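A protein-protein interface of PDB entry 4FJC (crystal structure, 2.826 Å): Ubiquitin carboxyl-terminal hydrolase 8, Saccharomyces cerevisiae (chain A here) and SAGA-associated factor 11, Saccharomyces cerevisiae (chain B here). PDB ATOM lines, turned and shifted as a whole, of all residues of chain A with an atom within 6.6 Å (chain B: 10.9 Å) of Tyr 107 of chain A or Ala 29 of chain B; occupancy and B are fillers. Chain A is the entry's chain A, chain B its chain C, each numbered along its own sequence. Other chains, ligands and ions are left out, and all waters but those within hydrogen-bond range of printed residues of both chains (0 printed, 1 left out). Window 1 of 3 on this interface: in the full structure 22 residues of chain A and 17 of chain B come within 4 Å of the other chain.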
ATOM      1  N   CYS A   9     -21.001   3.574  -4.575  1.00  0.00           N
ATOM      2  CA  CYS A   9     -19.982   2.847  -5.296  1.00  0.00           C
ATOM      3  C   CYS A   9     -19.931   3.357  -6.755  1.00  0.00           C
ATOM      4  O   CYS A   9     -20.884   3.181  -7.529  1.00  0.00           O
ATOM      5  CB  CYS A   9     -20.253   1.344  -5.258  1.00  0.00           C
ATOM      6  SG  CYS A   9     -18.894   0.383  -5.906  1.00  0.00           S
ATOM      7  N   ALA A  61     -16.240 -14.006   6.930  1.00  0.00           N
ATOM      8  CA  ALA A  61     -17.344 -13.978   5.987  1.00  0.00           C
ATOM      9  C   ALA A  61     -16.873 -14.592   4.697  1.00  0.00           C
ATOM     10  O   ALA A  61     -15.761 -14.357   4.239  1.00  0.00           O
ATOM     11  CB  ALA A  61     -17.865 -12.580   5.746  1.00  0.00           C
ATOM     12  N   PHE A  63     -17.952 -14.839   0.823  1.00  0.00           N
ATOM     13  CA  PHE A  63     -18.694 -14.085  -0.144  1.00  0.00           C
ATOM     14  C   PHE A  63     -19.017 -14.988  -1.309  1.00  0.00           C
ATOM     15  O   PHE A  63     -18.176 -15.816  -1.711  1.00  0.00           O
ATOM     16  CB  PHE A  63     -17.874 -12.893  -0.587  1.00  0.00           C
ATOM     17  CG  PHE A  63     -17.701 -11.887   0.493  1.00  0.00           C
ATOM     18  CD1 PHE A  63     -18.662 -10.927   0.711  1.00  0.00           C
ATOM     19  CD2 PHE A  63     -16.622 -11.941   1.327  1.00  0.00           C
ATOM     20  CE1 PHE A  63     -18.527 -10.012   1.723  1.00  0.00           C
ATOM     21  CE2 PHE A  63     -16.473 -11.029   2.338  1.00  0.00           C
ATOM     22  CZ  PHE A  63     -17.422 -10.055   2.528  1.00  0.00           C
ATOM     23  N   TRP A  74     -12.836 -14.133   3.652  1.00  0.00           N
ATOM     24  CA  TRP A  74     -12.307 -12.849   4.066  1.00  0.00           C
ATOM     25  C   TRP A  74     -10.981 -12.948   4.784  1.00  0.00           C
ATOM     26  O   TRP A  74     -10.020 -12.262   4.442  1.00  0.00           O
ATOM     27  CB  TRP A  74     -13.323 -12.177   4.967  1.00  0.00           C
ATOM     28  CG  TRP A  74     -12.820 -10.897   5.579  1.00  0.00           C
ATOM     29  CD1 TRP A  74     -12.108 -10.747   6.741  1.00  0.00           C
ATOM     30  CD2 TRP A  74     -12.962  -9.550   5.044  1.00  0.00           C
ATOM     31  NE1 TRP A  74     -11.810  -9.447   6.954  1.00  0.00           N
ATOM     32  CE2 TRP A  74     -12.292  -8.678   5.976  1.00  0.00           C
ATOM     33  CE3 TRP A  74     -13.554  -9.006   3.920  1.00  0.00           C
ATOM     34  CZ2 TRP A  74     -12.247  -7.318   5.796  1.00  0.00           C
ATOM     35  CZ3 TRP A  74     -13.510  -7.639   3.748  1.00  0.00           C
ATOM     36  CH2 TRP A  74     -12.866  -6.812   4.660  1.00  0.00           C
ATOM     37  N   GLY A  91     -19.270  -9.182  -4.467  1.00  0.00           N
ATOM     38  CA  GLY A  91     -19.503 -10.439  -3.766  1.00  0.00           C
ATOM     39  C   GLY A  91     -20.573 -10.273  -2.728  1.00  0.00           C
ATOM     40  O   GLY A  91     -20.722  -9.185  -2.176  1.00  0.00           O
ATOM     41  N   ILE A  92     -21.310 -11.346  -2.444  1.00  0.00           N
ATOM     42  CA  ILE A  92     -22.398 -11.282  -1.483  1.00  0.00           C
ATOM     43  C   ILE A  92     -22.106 -12.126  -0.247  1.00  0.00           C
ATOM     44  O   ILE A  92     -21.680 -13.274  -0.373  1.00  0.00           O
ATOM     45  CB  ILE A  92     -23.705 -11.778  -2.107  1.00  0.00           C
ATOM     46  CG1 ILE A  92     -23.968 -11.034  -3.413  1.00  0.00           C
ATOM     47  CG2 ILE A  92     -24.873 -11.579  -1.145  1.00  0.00           C
ATOM     48  CD1 ILE A  92     -25.437 -10.940  -3.780  1.00  0.00           C
ATOM     49  N   ASN A  93     -22.381 -11.564   0.935  1.00  0.00           N
ATOM     50  CA  ASN A  93     -22.014 -12.179   2.196  1.00  0.00           C
ATOM     51  C   ASN A  93     -23.037 -13.245   2.580  1.00  0.00           C
ATOM     52  O   ASN A  93     -24.206 -12.932   2.832  1.00  0.00           O
ATOM     53  CB  ASN A  93     -21.924 -11.084   3.275  1.00  0.00           C
ATOM     54  CG  ASN A  93     -21.744 -11.639   4.692  1.00  0.00           C
ATOM     55  OD1 ASN A  93     -22.394 -12.594   5.084  1.00  0.00           O
ATOM     56  ND2 ASN A  93     -20.864 -11.021   5.461  1.00  0.00           N
ATOM     57  N   ASN A  96     -25.692 -12.740   5.360  1.00  0.00           N
ATOM     58  CA  ASN A  96     -26.666 -11.623   5.393  1.00  0.00           C
ATOM     59  C   ASN A  96     -27.121 -11.053   4.051  1.00  0.00           C
ATOM     60  O   ASN A  96     -27.832 -10.076   4.027  1.00  0.00           O
ATOM     61  CB  ASN A  96     -26.116 -10.484   6.265  1.00  0.00           C
ATOM     62  CG  ASN A  96     -24.697 -10.086   5.875  1.00  0.00           C
ATOM     63  OD1 ASN A  96     -24.417  -9.860   4.726  1.00  0.00           O
ATOM     64  ND2 ASN A  96     -23.797 -10.033   6.847  1.00  0.00           N
ATOM     65  N   LEU A  98     -25.665  -9.292   1.856  1.00  0.00           N
ATOM     66  CA  LEU A  98     -25.251  -7.905   1.671  1.00  0.00           C
ATOM     67  C   LEU A  98     -24.142  -7.819   0.659  1.00  0.00           C
ATOM     68  O   LEU A  98     -23.186  -8.617   0.708  1.00  0.00           O
ATOM     69  CB  LEU A  98     -24.752  -7.319   2.964  1.00  0.00           C
ATOM     70  CG  LEU A  98     -25.859  -6.985   3.916  1.00  0.00           C
ATOM     71  CD1 LEU A  98     -25.254  -6.856   5.297  1.00  0.00           C
ATOM     72  CD2 LEU A  98     -26.519  -5.701   3.463  1.00  0.00           C
ATOM     73  N   LEU A  99     -24.274  -6.857  -0.253  1.00  0.00           N
ATOM     74  CA  LEU A  99     -23.418  -6.791  -1.414  1.00  0.00           C
ATOM     75  C   LEU A  99     -22.201  -5.940  -1.081  1.00  0.00           C
ATOM     76  O   LEU A  99     -22.353  -4.832  -0.529  1.00  0.00           O
ATOM     77  CB  LEU A  99     -24.171  -6.206  -2.602  1.00  0.00           C
ATOM     78  CG  LEU A  99     -23.383  -6.141  -3.917  1.00  0.00           C
ATOM     79  CD1 LEU A  99     -22.926  -7.514  -4.365  1.00  0.00           C
ATOM     80  CD2 LEU A  99     -24.224  -5.464  -4.989  1.00  0.00           C
ATOM     81  N   PHE A 100     -21.016  -6.460  -1.419  1.00  0.00           N
ATOM     82  CA  PHE A 100     -19.747  -5.848  -1.063  1.00  0.00           C
ATOM     83  C   PHE A 100     -18.912  -5.529  -2.301  1.00  0.00           C
ATOM     84  O   PHE A 100     -18.938  -6.298  -3.289  1.00  0.00           O
ATOM     85  CB  PHE A 100     -18.981  -6.804  -0.167  1.00  0.00           C
ATOM     86  CG  PHE A 100     -17.769  -6.206   0.439  1.00  0.00           C
ATOM     87  CD1 PHE A 100     -17.851  -5.474   1.604  1.00  0.00           C
ATOM     88  CD2 PHE A 100     -16.532  -6.362  -0.150  1.00  0.00           C
ATOM     89  CE1 PHE A 100     -16.706  -4.892   2.178  1.00  0.00           C
ATOM     90  CE2 PHE A 100     -15.374  -5.779   0.418  1.00  0.00           C
ATOM     91  CZ  PHE A 100     -15.462  -5.038   1.589  1.00  0.00           C
ATOM     92  N   CYS A 101     -18.167  -4.423  -2.270  1.00  0.00           N
ATOM     93  CA  CYS A 101     -17.331  -4.061  -3.410  1.00  0.00           C
ATOM     94  C   CYS A 101     -15.850  -4.164  -3.033  1.00  0.00           C
ATOM     95  O   CYS A 101     -15.374  -3.435  -2.181  1.00  0.00           O
ATOM     96  CB  CYS A 101     -17.666  -2.661  -3.915  1.00  0.00           C
ATOM     97  SG  CYS A 101     -16.446  -2.043  -5.097  1.00  0.00           S
ATOM     98  N   CYS A 104     -13.910  -0.646  -3.608  1.00  0.00           N
ATOM     99  CA  CYS A 104     -14.223   0.324  -2.585  1.00  0.00           C
ATOM    100  C   CYS A 104     -13.810  -0.179  -1.219  1.00  0.00           C
ATOM    101  O   CYS A 104     -13.749   0.597  -0.279  1.00  0.00           O
ATOM    102  CB  CYS A 104     -15.728   0.619  -2.535  1.00  0.00           C
ATOM    103  SG  CYS A 104     -16.368   1.393  -4.028  1.00  0.00           S
ATOM    104  N   GLU A 105     -13.577  -1.478  -1.089  1.00  0.00           N
ATOM    105  CA  GLU A 105     -13.475  -2.116   0.239  1.00  0.00           C
ATOM    106  C   GLU A 105     -14.597  -1.746   1.249  1.00  0.00           C
ATOM    107  O   GLU A 105     -14.338  -1.636   2.440  1.00  0.00           O
ATOM    108  CB  GLU A 105     -12.097  -1.872   0.825  1.00  0.00           C
ATOM    109  CG  GLU A 105     -11.022  -2.660   0.091  1.00  0.00           C
ATOM    110  CD  GLU A 105      -9.624  -2.385   0.622  1.00  0.00           C
ATOM    111  OE1 GLU A 105      -9.502  -1.439   1.418  1.00  0.00           O
ATOM    112  OE2 GLU A 105      -8.648  -3.082   0.241  1.00  0.00           O
ATOM    113  N   ASP A 106     -15.832  -1.586   0.760  1.00  0.00           N
ATOM    114  CA  ASP A 106     -16.999  -1.355   1.606  1.00  0.00           C
ATOM    115  C   ASP A 106     -18.204  -2.104   1.014  1.00  0.00           C
ATOM    116  O   ASP A 106     -18.096  -2.703  -0.034  1.00  0.00           O
ATOM    117  CB  ASP A 106     -17.287   0.154   1.723  1.00  0.00           C
ATOM    118  CG  ASP A 106     -18.107   0.514   2.958  1.00  0.00           C
ATOM    119  OD1 ASP A 106     -18.363  -0.363   3.819  1.00  0.00           O
ATOM    120  OD2 ASP A 106     -18.488   1.692   3.104  1.00  0.00           O
ATOM    121  N   TYR A 107     -19.319  -2.123   1.732  1.00  0.00           N
ATOM    122  CA  TYR A 107     -20.567  -2.686   1.251  1.00  0.00           C
ATOM    123  C   TYR A 107     -21.329  -1.623   0.494  1.00  0.00           C
ATOM    124  O   TYR A 107     -21.156  -0.412   0.748  1.00  0.00           O
ATOM    125  CB  TYR A 107     -21.453  -3.173   2.408  1.00  0.00           C
ATOM    126  CG  TYR A 107     -21.001  -4.478   2.983  1.00  0.00           C
ATOM    127  CD1 TYR A 107     -21.396  -5.684   2.416  1.00  0.00           C
ATOM    128  CD2 TYR A 107     -20.168  -4.516   4.072  1.00  0.00           C
ATOM    129  CE1 TYR A 107     -20.961  -6.885   2.914  1.00  0.00           C
ATOM    130  CE2 TYR A 107     -19.729  -5.726   4.590  1.00  0.00           C
ATOM    131  CZ  TYR A 107     -20.129  -6.904   4.005  1.00  0.00           C
ATOM    132  OH  TYR A 107     -19.682  -8.092   4.521  1.00  0.00           O
ATOM    133  N   ILE A 108     -22.195  -2.071  -0.411  1.00  0.00           N
ATOM    134  CA  ILE A 108     -23.122  -1.178  -1.066  1.00  0.00           C
ATOM    135  C   ILE A 108     -24.456  -1.194  -0.322  1.00  0.00           C
ATOM    136  O   ILE A 108     -25.330  -2.067  -0.531  1.00  0.00           O
ATOM    137  CB  ILE A 108     -23.283  -1.580  -2.505  1.00  0.00           C
ATOM    138  CG1 ILE A 108     -21.904  -1.586  -3.137  1.00  0.00           C
ATOM    139  CG2 ILE A 108     -24.282  -0.655  -3.193  1.00  0.00           C
ATOM    140  CD1 ILE A 108     -21.974  -1.758  -4.615  1.00  0.00           C
ATOM    141  N   GLY A 109     -24.583  -0.222   0.573  1.00  0.00           N
ATOM    142  CA  GLY A 109     -25.640  -0.239   1.570  1.00  0.00           C
ATOM    143  C   GLY A 109     -26.786   0.677   1.238  1.00  0.00           C
ATOM    144  O   GLY A 109     -27.935   0.453   1.710  1.00  0.00           O
ATOM    145  N   ASN A 110     -26.492   1.655   0.371  1.00  0.00           N
ATOM    146  CA  ASN A 110     -27.344   2.833   0.206  1.00  0.00           C
ATOM    147  C   ASN A 110     -27.913   3.013  -1.159  1.00  0.00           C
ATOM    148  O   ASN A 110     -28.320   4.093  -1.506  1.00  0.00           O
ATOM    149  CB  ASN A 110     -26.558   4.099   0.575  1.00  0.00           C
ATOM    150  CG  ASN A 110     -25.295   4.272  -0.235  1.00  0.00           C
ATOM    151  OD1 ASN A 110     -24.976   3.439  -1.084  1.00  0.00           O
ATOM    152  ND2 ASN A 110     -24.559   5.342   0.034  1.00  0.00           N
ATOM    153  N   LEU B  20     -16.022 -17.147  15.506  1.00  0.00           N
ATOM    154  CA  LEU B  20     -16.202 -15.867  16.180  1.00  0.00           C
ATOM    155  C   LEU B  20     -16.017 -14.678  15.237  1.00  0.00           C
ATOM    156  O   LEU B  20     -16.738 -13.699  15.332  1.00  0.00           O
ATOM    157  CB  LEU B  20     -15.223 -15.748  17.346  1.00  0.00           C
ATOM    158  CG  LEU B  20     -15.547 -16.460  18.663  1.00  0.00           C
ATOM    159  CD1 LEU B  20     -14.338 -16.276  19.590  1.00  0.00           C
ATOM    160  CD2 LEU B  20     -16.841 -15.936  19.275  1.00  0.00           C
ATOM    161  N   THR B  21     -15.018 -14.766  14.358  1.00  0.00           N
ATOM    162  CA  THR B  21     -14.752 -13.737  13.355  1.00  0.00           C
ATOM    163  C   THR B  21     -15.902 -13.642  12.320  1.00  0.00           C
ATOM    164  O   THR B  21     -16.180 -12.555  11.816  1.00  0.00           O
ATOM    165  CB  THR B  21     -13.390 -13.977  12.640  1.00  0.00           C
ATOM    166  OG1 THR B  21     -13.320 -15.318  12.149  1.00  0.00           O
ATOM    167  CG2 THR B  21     -12.223 -13.735  13.600  1.00  0.00           C
ATOM    168  N   THR B  22     -16.580 -14.750  12.014  1.00  0.00           N
ATOM    169  CA  THR B  22     -17.708 -14.681  11.094  1.00  0.00           C
ATOM    170  C   THR B  22     -18.831 -13.870  11.731  1.00  0.00           C
ATOM    171  O   THR B  22     -19.421 -12.995  11.097  1.00  0.00           O
ATOM    172  CB  THR B  22     -18.256 -16.067  10.679  1.00  0.00           C
ATOM    173  OG1 THR B  22     -17.237 -16.819  10.001  1.00  0.00           O
ATOM    174  CG2 THR B  22     -19.452 -15.907   9.748  1.00  0.00           C
ATOM    175  N   LEU B  23     -19.108 -14.141  12.992  1.00  0.00           N
ATOM    176  CA  LEU B  23     -20.220 -13.511  13.678  1.00  0.00           C
ATOM    177  C   LEU B  23     -19.970 -12.010  13.822  1.00  0.00           C
ATOM    178  O   LEU B  23     -20.902 -11.186  13.703  1.00  0.00           O
ATOM    179  CB  LEU B  23     -20.407 -14.140  15.052  1.00  0.00           C
ATOM    180  CG  LEU B  23     -21.831 -14.419  15.515  1.00  0.00           C
ATOM    181  CD1 LEU B  23     -21.818 -14.916  16.956  1.00  0.00           C
ATOM    182  CD2 LEU B  23     -22.705 -13.188  15.368  1.00  0.00           C
ATOM    183  N   ILE B  24     -18.719 -11.641  14.080  1.00  0.00           N
ATOM    184  CA  ILE B  24     -18.404 -10.237  14.281  1.00  0.00           C
ATOM    185  C   ILE B  24     -18.599  -9.542  12.938  1.00  0.00           C
ATOM    186  O   ILE B  24     -19.196  -8.440  12.850  1.00  0.00           O
ATOM    187  CB  ILE B  24     -16.961 -10.024  14.815  1.00  0.00           C
ATOM    188  CG1 ILE B  24     -16.862 -10.617  16.238  1.00  0.00           C
ATOM    189  CG2 ILE B  24     -16.593  -8.543  14.807  1.00  0.00           C
ATOM    190  CD1 ILE B  24     -15.469 -10.848  16.796  1.00  0.00           C
ATOM    191  N   GLN B  25     -18.119 -10.202  11.888  1.00  0.00           N
ATOM    192  CA  GLN B  25     -18.107  -9.556  10.609  1.00  0.00           C
ATOM    193  C   GLN B  25     -19.536  -9.439  10.047  1.00  0.00           C
ATOM    194  O   GLN B  25     -19.806  -8.566   9.226  1.00  0.00           O
ATOM    195  CB  GLN B  25     -17.183 -10.285   9.655  1.00  0.00           C
ATOM    196  CG  GLN B  25     -15.722 -10.067   9.945  1.00  0.00           C
ATOM    197  CD  GLN B  25     -14.848 -11.056   9.205  1.00  0.00           C
ATOM    198  OE1 GLN B  25     -13.866 -11.576   9.751  1.00  0.00           O
ATOM    199  NE2 GLN B  25     -15.187 -11.304   7.940  1.00  0.00           N
ATOM    200  N   ASP B  26     -20.429 -10.322  10.492  1.00  0.00           N
ATOM    201  CA  ASP B  26     -21.854 -10.275  10.166  1.00  0.00           C
ATOM    202  C   ASP B  26     -22.454  -9.024  10.794  1.00  0.00           C
ATOM    203  O   ASP B  26     -23.097  -8.216  10.130  1.00  0.00           O
ATOM    204  CB  ASP B  26     -22.536 -11.552  10.736  1.00  0.00           C
ATOM    205  CG  ASP B  26     -23.994 -11.740  10.276  1.00  0.00           C
ATOM    206  OD1 ASP B  26     -24.469 -10.976   9.420  1.00  0.00           O
ATOM    207  OD2 ASP B  26     -24.666 -12.668  10.769  1.00  0.00           O
ATOM    208  N   ILE B  27     -22.233  -8.897  12.095  1.00  0.00           N
ATOM    209  CA  ILE B  27     -22.817  -7.836  12.923  1.00  0.00           C
ATOM    210  C   ILE B  27     -22.321  -6.459  12.474  1.00  0.00           C
ATOM    211  O   ILE B  27     -23.113  -5.568  12.260  1.00  0.00           O
ATOM    212  CB  ILE B  27     -22.478  -8.068  14.422  1.00  0.00           C
ATOM    213  CG1 ILE B  27     -23.200  -9.300  14.944  1.00  0.00           C
ATOM    214  CG2 ILE B  27     -22.859  -6.872  15.278  1.00  0.00           C
ATOM    215  CD1 ILE B  27     -22.670  -9.761  16.278  1.00  0.00           C
ATOM    216  N   VAL B  28     -21.010  -6.321  12.298  1.00  0.00           N
ATOM    217  CA  VAL B  28     -20.412  -5.081  11.806  1.00  0.00           C
ATOM    218  C   VAL B  28     -20.921  -4.765  10.404  1.00  0.00           C
ATOM    219  O   VAL B  28     -21.298  -3.629  10.141  1.00  0.00           O
ATOM    220  CB  VAL B  28     -18.850  -5.127  11.826  1.00  0.00           C
ATOM    221  CG1 VAL B  28     -18.269  -3.961  11.040  1.00  0.00           C
ATOM    222  CG2 VAL B  28     -18.319  -5.100  13.255  1.00  0.00           C
ATOM    223  N   ALA B  29     -20.973  -5.750   9.517  1.00  0.00           N
ATOM    224  CA  ALA B  29     -21.578  -5.527   8.204  1.00  0.00           C
ATOM    225  C   ALA B  29     -22.962  -4.977   8.350  1.00  0.00           C
ATOM    226  O   ALA B  29     -23.372  -4.121   7.589  1.00  0.00           O
ATOM    227  CB  ALA B  29     -21.640  -6.797   7.368  1.00  0.00           C
ATOM    228  N   ARG B  30     -23.712  -5.458   9.322  1.00  0.00           N
ATOM    229  CA  ARG B  30     -25.095  -5.055   9.383  1.00  0.00           C
ATOM    230  C   ARG B  30     -25.255  -3.686   9.928  1.00  0.00           C
ATOM    231  O   ARG B  30     -26.279  -3.067   9.702  1.00  0.00           O
ATOM    232  CB  ARG B  30     -25.896  -5.991  10.244  1.00  0.00           C
ATOM    233  CG  ARG B  30     -26.289  -7.283   9.573  1.00  0.00           C
ATOM    234  CD  ARG B  30     -26.671  -8.237  10.680  1.00  0.00           C
ATOM    235  NE  ARG B  30     -26.739  -9.589  10.201  1.00  0.00           N
ATOM    236  CZ  ARG B  30     -27.828 -10.132   9.707  1.00  0.00           C
ATOM    237  NH1 ARG B  30     -28.943  -9.436   9.615  1.00  0.00           N
ATOM    238  NH2 ARG B  30     -27.788 -11.387   9.311  1.00  0.00           N
ATOM    239  N   GLU B  31     -24.270  -3.230  10.682  1.00  0.00           N
ATOM    240  CA  GLU B  31     -24.339  -1.930  11.331  1.00  0.00           C
ATOM    241  C   GLU B  31     -23.811  -0.867  10.413  1.00  0.00           C
ATOM    242  O   GLU B  31     -24.332   0.253  10.412  1.00  0.00           O
ATOM    243  CB  GLU B  31     -23.509  -1.906  12.607  1.00  0.00           C
ATOM    244  CG  GLU B  31     -24.075  -2.714  13.758  1.00  0.00           C
ATOM    245  CD  GLU B  31     -25.288  -2.082  14.412  1.00  0.00           C
ATOM    246  OE1 GLU B  31     -25.564  -0.845  14.245  1.00  0.00           O
ATOM    247  OE2 GLU B  31     -25.961  -2.852  15.144  1.00  0.00           O
ATOM    248  N   THR B  32     -22.771  -1.209   9.647  1.00  0.00           N
ATOM    249  CA  THR B  32     -22.088  -0.220   8.801  1.00  0.00           C
ATOM    250  C   THR B  32     -22.980   0.175   7.643  1.00  0.00           C
ATOM    251  O   THR B  32     -23.069   1.354   7.289  1.00  0.00           O
ATOM    252  CB  THR B  32     -20.716  -0.711   8.253  1.00  0.00           C
ATOM    253  OG1 THR B  32     -20.887  -1.890   7.454  1.00  0.00           O
ATOM    254  CG2 THR B  32     -19.737  -1.004   9.385  1.00  0.00           C
ATOM    255  N   THR B  33     -23.642  -0.824   7.068  1.00  0.00           N
ATOM    256  CA  THR B  33     -24.527  -0.627   5.925  1.00  0.00           C
ATOM    257  C   THR B  33     -25.751   0.150   6.353  1.00  0.00           C
ATOM    258  O   THR B  33     -26.149   1.127   5.743  1.00  0.00           O
ATOM    259  CB  THR B  33     -24.989  -1.979   5.381  1.00  0.00           C
ATOM    260  OG1 THR B  33     -25.475  -2.774   6.465  1.00  0.00           O
ATOM    261  CG2 THR B  33     -23.836  -2.724   4.724  1.00  0.00           C
ATOM    262  N   GLN B  34     -26.347  -0.303   7.433  1.00  0.00           N
ATOM    263  CA  GLN B  34     -27.584   0.249   7.905  1.00  0.00           C
ATOM    264  C   GLN B  34     -27.366   1.741   8.168  1.00  0.00           C
ATOM    265  O   GLN B  34     -28.282   2.548   8.000  1.00  0.00           O
ATOM    266  CB  GLN B  34     -27.961  -0.522   9.168  1.00  0.00           C
ATOM    267  CG  GLN B  34     -29.329  -0.290   9.771  1.00  0.00           C
ATOM    268  CD  GLN B  34     -29.377  -0.702  11.240  1.00  0.00           C
ATOM    269  OE1 GLN B  34     -28.934  -1.800  11.601  1.00  0.00           O
ATOM    270  NE2 GLN B  34     -29.898   0.183  12.095  1.00  0.00           N
ATOM    271  N   GLN B  35     -26.150   2.100   8.581  1.00  0.00           N
ATOM    272  CA  GLN B  35     -25.811   3.467   8.972  1.00  0.00           C
ATOM    273  C   GLN B  35     -25.411   4.290   7.741  1.00  0.00           C
ATOM    274  O   GLN B  35     -25.712   5.469   7.659  1.00  0.00           O
ATOM    275  CB  GLN B  35     -24.669   3.417  10.003  1.00  0.00           C
ATOM    276  CG  GLN B  35     -24.165   4.743  10.528  1.00  0.00           C
ATOM    277  CD  GLN B  35     -25.240   5.560  11.217  1.00  0.00           C
ATOM    278  OE1 GLN B  35     -26.322   5.059  11.554  1.00  0.00           O
ATOM    279  NE2 GLN B  35     -24.942   6.828  11.444  1.00  0.00           N
ATOM    280  N   GLN B  36     -24.726   3.664   6.793  1.00  0.00           N
ATOM    281  CA  GLN B  36     -24.489   4.272   5.495  1.00  0.00           C
ATOM    282  C   GLN B  36     -25.827   4.719   4.893  1.00  0.00           C
ATOM    283  O   GLN B  36     -25.970   5.857   4.482  1.00  0.00           O
ATOM    284  CB  GLN B  36     -23.753   3.284   4.557  1.00  0.00           C
ATOM    285  CG  GLN B  36     -23.313   3.877   3.237  1.00  0.00           C
ATOM    286  CD  GLN B  36     -22.816   2.842   2.226  1.00  0.00           C
ATOM    287  OE1 GLN B  36     -23.526   1.913   1.880  1.00  0.00           O
ATOM    288  NE2 GLN B  36     -21.618   3.042   1.700  1.00  0.00           N
ATOM    289  N   LEU B  37     -26.798   3.810   4.858  1.00  0.00           N
ATOM    290  CA  LEU B  37     -28.120   4.092   4.329  1.00  0.00           C
ATOM    291  C   LEU B  37     -28.743   5.302   4.999  1.00  0.00           C
ATOM    292  O   LEU B  37     -29.244   6.156   4.303  1.00  0.00           O
ATOM    293  CB  LEU B  37     -29.061   2.897   4.513  1.00  0.00           C
ATOM    294  CG  LEU B  37     -30.514   3.142   4.053  1.00  0.00           C
ATOM    295  CD1 LEU B  37     -30.473   3.433   2.563  1.00  0.00           C
ATOM    296  CD2 LEU B  37     -31.487   2.004   4.332  1.00  0.00           C
ATOM    297  N   THR B  40     -26.875   8.683   3.852  1.00  0.00           N
ATOM    298  CA  THR B  40     -27.228   8.996   2.464  1.00  0.00           C
ATOM    299  C   THR B  40     -28.694   9.437   2.339  1.00  0.00           C
ATOM    300  O   THR B  40     -29.040  10.269   1.523  1.00  0.00           O
ATOM    301  CB  THR B  40     -27.040   7.744   1.586  1.00  0.00           C
ATOM    302  OG1 THR B  40     -25.957   6.964   2.104  1.00  0.00           O
ATOM    303  CG2 THR B  40     -26.756   8.099   0.153  1.00  0.00           C
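Asn 93 of chain A touches none of the printed residues of chain B. No residue of chain B comes within 4 Å of Leu 98 of chain A. Phe 100 of chain A touches none of the printed residues of chain B. Asp 106 of chain A touches just one residue of chain B: Gln 36. Of chain B, only Ala 29, Thr 33 and Gln 36 come within 4 Å of Tyr 107 of chain A. Ile 108 of chain A touches just one residue of chain B: Gln 36 (3.9 Å). Of the printed residues of chain B, Asn 110 of chain A touches Gln 36, Leu 37 and Thr 40. Thr 22 of chain B touches none of the printed residues of chain A. Printed residues of chain A within 4 Å of Gln 25 of chain B: Ala 61 and Trp 74. Ala 29 of chain B touches just these residues of chain A: Asn 96 (3.9 Å) and Tyr 107 (3.5 Å). Glu 31 of chain B touches none of the printed residues of chain A. Of the printed residues of chain A, Gln 36 of chain B touches Asp 106, Tyr 107, Ile 108, Gly 109 and Asn 110. Printed residues of chain A within 4 Å of Leu 37 of chain B: Gly 109 (3.9 Å) and Asn 110 (3.96 Å). The nearest residue of chain B that does not touch Tyr 107 of chain A is Thr 32 of chain B (4.3 Å). The nearest printed residue of chain B that does not touch Gly 109 of chain A is Thr 33 of chain B (4.2 Å).
The side-chain amide oxygen (OD1) of Asn 96 of chain A lies close to the backbone NH (N) of Leu 98 of chain A, at 3.2 Å. O of Leu 99 of chain A lies within hydrogen-bond range of N of Ile 108 of chain A. The backbone NH of Cys 101 of chain A lies within hydrogen-bond range of the backbone carbonyl oxygen of Asp 106 of chain A. The side-chain carboxylate (OD1) of Asp 26 of chain B lies within salt-bridge range of the guanidinium group (NE) of Arg 30 of chain B. The side-chain hydroxyl of Thr 33 of chain B is in hydrogen-bond range of the backbone carbonyl oxygen of Ala 29 of chain B (2.7 Å). O of Gln 36 of chain B is in hydrogen-bond range of OG1 of Thr 40 of chain B (2.6 Å).
Among the printed residues, merely in contact across the chains: Trp 74 of chain A with Gln 25 of chain B, Tyr 107 of chain A with Thr 33 of chain B, Tyr 107 of chain A with Gln 36 of chain B, Tyr 107 of chain A with Ala 29 of chain B, Asn 96 of chain A with Arg 30 of chain B, Asp 106 of chain A with Gln 36 of chain B, Gly 109 of chain A with Leu 37 of chain B, Ile 108 of chain A with Gln 36 of chain B, Asn 96 of chain A with Ala 29 of chain B and Asn 110 of chain A with Leu 37 of chain B.
Of the 19 printed residues of chain A, 8 touch a printed residue of chain B. Of the 19 printed residues of chain B, 8 touch a printed residue of chain A. Hydrophobic or aromatic side chains of chain B that line the printed part of chain A: Ala 29 and Leu 37. Among the printed residues, 15 pairs touch across the chains. Among the printed residues, no Asp or Glu carboxylate lies within 4 Å of a Lys or Arg side-chain nitrogen of the other chain.
N of Ala 61 of chain A sits close to NE2 of Gln 25 of chain B (3.1 Å). OD1 of Asp 26 of chain B sits at hydrogen-bond distance from ND2 of Asn 96 of chain A (2.8 Å). N of Gly 109 of chain A lies within hydrogen-bond range of OE1 of Gln 36 of chain B (2.7 Å). N of Asn 110 of chain A lies within hydrogen-bond range of OE1 of Gln 36 of chain B (3.3 Å). The side-chain hydroxyl (OG1) of Thr 40 of chain B sits at hydrogen-bond distance from the side-chain amide nitrogen (ND2) of Asn 110 of chain A, at 3.0 Å.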
